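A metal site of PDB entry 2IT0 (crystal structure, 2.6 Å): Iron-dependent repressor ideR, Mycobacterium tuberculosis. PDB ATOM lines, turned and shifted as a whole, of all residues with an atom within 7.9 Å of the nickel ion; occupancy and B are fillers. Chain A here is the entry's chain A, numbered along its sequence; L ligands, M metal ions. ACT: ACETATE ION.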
ATOM      1  N   ARG A  13     -31.644 -16.666 -14.983  1.00  0.00           N
ATOM      2  CA  ARG A  13     -30.617 -17.552 -15.533  1.00  0.00           C
ATOM      3  C   ARG A  13     -29.866 -18.221 -14.398  1.00  0.00           C
ATOM      4  O   ARG A  13     -29.520 -19.393 -14.486  1.00  0.00           O
ATOM      5  CB  ARG A  13     -29.662 -16.775 -16.450  1.00  0.00           C
ATOM      6  CG  ARG A  13     -29.013 -17.606 -17.589  1.00  0.00           C
ATOM      7  CD  ARG A  13     -27.584 -18.026 -17.272  1.00  0.00           C
ATOM      8  NE  ARG A  13     -26.655 -16.904 -17.383  1.00  0.00           N
ATOM      9  CZ  ARG A  13     -25.574 -16.751 -16.626  1.00  0.00           C
ATOM     10  NH1 ARG A  13     -25.272 -17.646 -15.700  1.00  0.00           N
ATOM     11  NH2 ARG A  13     -24.783 -15.684 -16.786  1.00  0.00           N
ATOM     12  N   ASP A  17     -29.439 -22.060 -13.792  1.00  0.00           N
ATOM     13  CA  ASP A  17     -28.120 -22.661 -13.590  1.00  0.00           C
ATOM     14  C   ASP A  17     -28.127 -23.628 -12.407  1.00  0.00           C
ATOM     15  O   ASP A  17     -27.514 -24.699 -12.476  1.00  0.00           O
ATOM     16  CB  ASP A  17     -27.051 -21.588 -13.354  1.00  0.00           C
ATOM     17  CG  ASP A  17     -26.347 -21.173 -14.637  1.00  0.00           C
ATOM     18  OD1 ASP A  17     -26.104 -22.042 -15.495  1.00  0.00           O
ATOM     19  OD2 ASP A  17     -26.012 -19.983 -14.762  1.00  0.00           O
ATOM     20  N   MET A  76     -30.495 -18.508 -21.270  1.00  0.00           N
ATOM     21  CA  MET A  76     -29.544 -19.604 -21.255  1.00  0.00           C
ATOM     22  C   MET A  76     -29.162 -20.026 -22.692  1.00  0.00           C
ATOM     23  O   MET A  76     -28.017 -20.353 -22.985  1.00  0.00           O
ATOM     24  CB  MET A  76     -30.172 -20.767 -20.501  1.00  0.00           C
ATOM     25  CG  MET A  76     -29.351 -22.040 -20.489  1.00  0.00           C
ATOM     26  SD  MET A  76     -27.857 -21.796 -19.532  1.00  0.00           S
ATOM     27  CE  MET A  76     -28.460 -22.184 -17.886  1.00  0.00           C
ATOM     28  N   HIS A  79     -27.001 -17.389 -24.151  1.00  0.00           N
ATOM     29  CA  HIS A  79     -25.713 -17.434 -23.481  1.00  0.00           C
ATOM     30  C   HIS A  79     -24.787 -18.412 -24.209  1.00  0.00           C
ATOM     31  O   HIS A  79     -23.689 -18.054 -24.659  1.00  0.00           O
ATOM     32  CB  HIS A  79     -25.901 -17.829 -22.006  1.00  0.00           C
ATOM     33  CG  HIS A  79     -24.624 -17.989 -21.239  1.00  0.00           C
ATOM     34  ND1 HIS A  79     -23.859 -16.918 -20.833  1.00  0.00           N
ATOM     35  CD2 HIS A  79     -23.978 -19.098 -20.800  1.00  0.00           C
ATOM     36  CE1 HIS A  79     -22.797 -17.358 -20.175  1.00  0.00           C
ATOM     37  NE2 HIS A  79     -22.844 -18.679 -20.145  1.00  0.00           N
ATOM     38  N   ARG A  80     -25.267 -19.637 -24.345  1.00  0.00           N
ATOM     39  CA  ARG A  80     -24.463 -20.706 -24.896  1.00  0.00           C
ATOM     40  C   ARG A  80     -24.284 -20.620 -26.404  1.00  0.00           C
ATOM     41  O   ARG A  80     -23.226 -20.988 -26.924  1.00  0.00           O
ATOM     42  CB  ARG A  80     -25.034 -22.038 -24.440  1.00  0.00           C
ATOM     43  CG  ARG A  80     -25.061 -22.069 -22.929  1.00  0.00           C
ATOM     44  CD  ARG A  80     -25.445 -23.386 -22.353  1.00  0.00           C
ATOM     45  NE  ARG A  80     -25.347 -23.264 -20.913  1.00  0.00           N
ATOM     46  CZ  ARG A  80     -25.651 -24.215 -20.038  1.00  0.00           C
ATOM     47  NH1 ARG A  80     -26.099 -25.396 -20.456  1.00  0.00           N
ATOM     48  NH2 ARG A  80     -25.523 -23.984 -18.746  1.00  0.00           N
ATOM     49  N   GLU A  83     -21.553 -18.419 -26.699  1.00  0.00           N
ATOM     50  CA  GLU A  83     -20.327 -19.066 -26.283  1.00  0.00           C
ATOM     51  C   GLU A  83     -19.733 -19.826 -27.457  1.00  0.00           C
ATOM     52  O   GLU A  83     -18.541 -19.751 -27.714  1.00  0.00           O
ATOM     53  CB  GLU A  83     -20.547 -19.966 -25.055  1.00  0.00           C
ATOM     54  CG  GLU A  83     -20.596 -19.168 -23.719  1.00  0.00           C
ATOM     55  CD  GLU A  83     -20.947 -20.007 -22.501  1.00  0.00           C
ATOM     56  OE1 GLU A  83     -21.126 -21.235 -22.646  1.00  0.00           O
ATOM     57  OE2 GLU A  83     -21.041 -19.439 -21.380  1.00  0.00           O
ATOM     58  N   VAL A  97     -14.558 -16.300 -22.299  1.00  0.00           N
ATOM     59  CA  VAL A  97     -15.753 -16.524 -23.137  1.00  0.00           C
ATOM     60  C   VAL A  97     -17.072 -16.465 -22.358  1.00  0.00           C
ATOM     61  O   VAL A  97     -18.020 -15.800 -22.776  1.00  0.00           O
ATOM     62  CB  VAL A  97     -15.679 -17.815 -23.988  1.00  0.00           C
ATOM     63  CG1 VAL A  97     -14.286 -17.980 -24.603  1.00  0.00           C
ATOM     64  CG2 VAL A  97     -16.044 -19.015 -23.162  1.00  0.00           C
ATOM     65  N   HIS A  98     -17.141 -17.165 -21.234  1.00  0.00           N
ATOM     66  CA  HIS A  98     -18.333 -17.113 -20.420  1.00  0.00           C
ATOM     67  C   HIS A  98     -18.642 -15.674 -20.032  1.00  0.00           C
ATOM     68  O   HIS A  98     -19.755 -15.197 -20.236  1.00  0.00           O
ATOM     69  CB  HIS A  98     -18.189 -17.992 -19.178  1.00  0.00           C
ATOM     70  CG  HIS A  98     -19.291 -17.789 -18.193  1.00  0.00           C
ATOM     71  ND1 HIS A  98     -20.548 -18.309 -18.380  1.00  0.00           N
ATOM     72  CD2 HIS A  98     -19.330 -17.068 -17.047  1.00  0.00           C
ATOM     73  CE1 HIS A  98     -21.324 -17.943 -17.369  1.00  0.00           C
ATOM     74  NE2 HIS A  98     -20.604 -17.187 -16.547  1.00  0.00           N
ATOM     75  N   ALA A  99     -17.657 -14.983 -19.462  1.00  0.00           N
ATOM     76  CA  ALA A  99     -17.821 -13.576 -19.104  1.00  0.00           C
ATOM     77  C   ALA A  99     -18.413 -12.786 -20.252  1.00  0.00           C
ATOM     78  O   ALA A  99     -19.405 -12.087 -20.062  1.00  0.00           O
ATOM     79  CB  ALA A  99     -16.516 -12.962 -18.664  1.00  0.00           C
ATOM     80  N   ALA A 101     -20.064 -13.837 -22.834  1.00  0.00           N
ATOM     81  CA  ALA A 101     -21.413 -14.332 -23.078  1.00  0.00           C
ATOM     82  C   ALA A 101     -22.407 -13.842 -22.019  1.00  0.00           C
ATOM     83  O   ALA A 101     -23.548 -13.496 -22.348  1.00  0.00           O
ATOM     84  CB  ALA A 101     -21.419 -15.850 -23.168  1.00  0.00           C
ATOM     85  N   CYS A 102     -21.958 -13.780 -20.777  1.00  0.00           N
ATOM     86  CA  CYS A 102     -22.774 -13.284 -19.680  1.00  0.00           C
ATOM     87  C   CYS A 102     -23.367 -11.912 -19.976  1.00  0.00           C
ATOM     88  O   CYS A 102     -24.420 -11.526 -19.432  1.00  0.00           O
ATOM     89  CB  CYS A 102     -21.951 -13.220 -18.386  1.00  0.00           C
ATOM     90  SG  CYS A 102     -22.898 -12.818 -16.959  1.00  0.00           S
ATOM     91  N   GLU A 105     -25.720 -12.585 -23.762  1.00  0.00           N
ATOM     92  CA  GLU A 105     -27.009 -13.208 -23.470  1.00  0.00           C
ATOM     93  C   GLU A 105     -28.157 -12.215 -23.321  1.00  0.00           C
ATOM     94  O   GLU A 105     -29.321 -12.573 -23.447  1.00  0.00           O
ATOM     95  CB  GLU A 105     -26.923 -14.055 -22.196  1.00  0.00           C
ATOM     96  CG  GLU A 105     -26.572 -13.271 -20.938  1.00  0.00           C
ATOM     97  CD  GLU A 105     -26.311 -14.166 -19.740  1.00  0.00           C
ATOM     98  OE1 GLU A 105     -26.630 -15.379 -19.825  1.00  0.00           O
ATOM     99  OE2 GLU A 105     -25.785 -13.647 -18.717  1.00  0.00           O
ATOM    100  N   SER A 126     -22.780 -25.883 -25.753  1.00  0.00           N
ATOM    101  CA  SER A 126     -21.778 -24.849 -25.587  1.00  0.00           C
ATOM    102  C   SER A 126     -20.414 -25.511 -25.632  1.00  0.00           C
ATOM    103  O   SER A 126     -20.302 -26.700 -25.370  1.00  0.00           O
ATOM    104  CB  SER A 126     -21.951 -24.159 -24.234  1.00  0.00           C
ATOM    105  OG  SER A 126     -21.173 -24.831 -23.264  1.00  0.00           O
ATOM    106  N   PRO A 127     -19.370 -24.739 -25.940  1.00  0.00           N
ATOM    107  CA  PRO A 127     -17.992 -25.242 -25.956  1.00  0.00           C
ATOM    108  C   PRO A 127     -17.557 -25.838 -24.620  1.00  0.00           C
ATOM    109  O   PRO A 127     -16.566 -26.563 -24.558  1.00  0.00           O
ATOM    110  CB  PRO A 127     -17.166 -23.998 -26.283  1.00  0.00           C
ATOM    111  CG  PRO A 127     -18.055 -22.846 -25.977  1.00  0.00           C
ATOM    112  CD  PRO A 127     -19.423 -23.324 -26.326  1.00  0.00           C
ATOM    113  N   PHE A 128     -18.278 -25.561 -23.550  1.00  0.00           N
ATOM    114  CA  PHE A 128     -17.916 -26.114 -22.255  1.00  0.00           C
ATOM    115  C   PHE A 128     -18.495 -27.506 -22.011  1.00  0.00           C
ATOM    116  O   PHE A 128     -18.202 -28.121 -20.996  1.00  0.00           O
ATOM    117  CB  PHE A 128     -18.327 -25.176 -21.138  1.00  0.00           C
ATOM    118  CG  PHE A 128     -17.638 -23.839 -21.185  1.00  0.00           C
ATOM    119  CD1 PHE A 128     -18.179 -22.791 -21.924  1.00  0.00           C
ATOM    120  CD2 PHE A 128     -16.457 -23.628 -20.486  1.00  0.00           C
ATOM    121  CE1 PHE A 128     -17.551 -21.562 -21.961  1.00  0.00           C
ATOM    122  CE2 PHE A 128     -15.828 -22.399 -20.523  1.00  0.00           C
ATOM    123  CZ  PHE A 128     -16.369 -21.366 -21.264  1.00  0.00           C
ATOM    124  N   ASN A 130     -21.838 -28.176 -21.838  1.00  0.00           N
ATOM    125  CA  ASN A 130     -23.232 -27.975 -21.411  1.00  0.00           C
ATOM    126  C   ASN A 130     -24.241 -27.874 -22.553  1.00  0.00           C
ATOM    127  O   ASN A 130     -23.984 -27.183 -23.548  1.00  0.00           O
ATOM    128  CB  ASN A 130     -23.324 -26.720 -20.555  1.00  0.00           C
ATOM    129  CG  ASN A 130     -22.277 -26.684 -19.465  1.00  0.00           C
ATOM    130  OD1 ASN A 130     -21.447 -25.771 -19.422  1.00  0.00           O
ATOM    131  ND2 ASN A 130     -22.298 -27.674 -18.593  1.00  0.00           N
HETATM  132  C   ACT L   1     -21.395 -21.978 -18.470  1.00  0.00           C
HETATM  133  O   ACT L   1     -21.839 -20.995 -17.811  1.00  0.00           O
HETATM  134  OXT ACT L   1     -21.846 -22.093 -19.647  1.00  0.00           O
HETATM  135  CH3 ACT L   1     -20.387 -22.925 -17.860  1.00  0.00           C
HETATM  136 NI    NI M   1     -21.309 -19.814 -19.483  1.00  0.00          NI
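The nickel ion is bound by the side-chain carboxylate (OE2) of Glu 83 (2.0 Å), a ring nitrogen (ND1) of His 98 (2.0 Å), a ring nitrogen (NE2) of His 79 (2.0 Å), an oxygen (O) of the ligand (2.1 Å) and an oxygen (OXT) of the ligand (2.3 Å).
A ring nitrogen (ND1) of His 79 sits at hydrogen-bond distance from the side-chain carboxylate of Glu 105 (3.3 Å).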
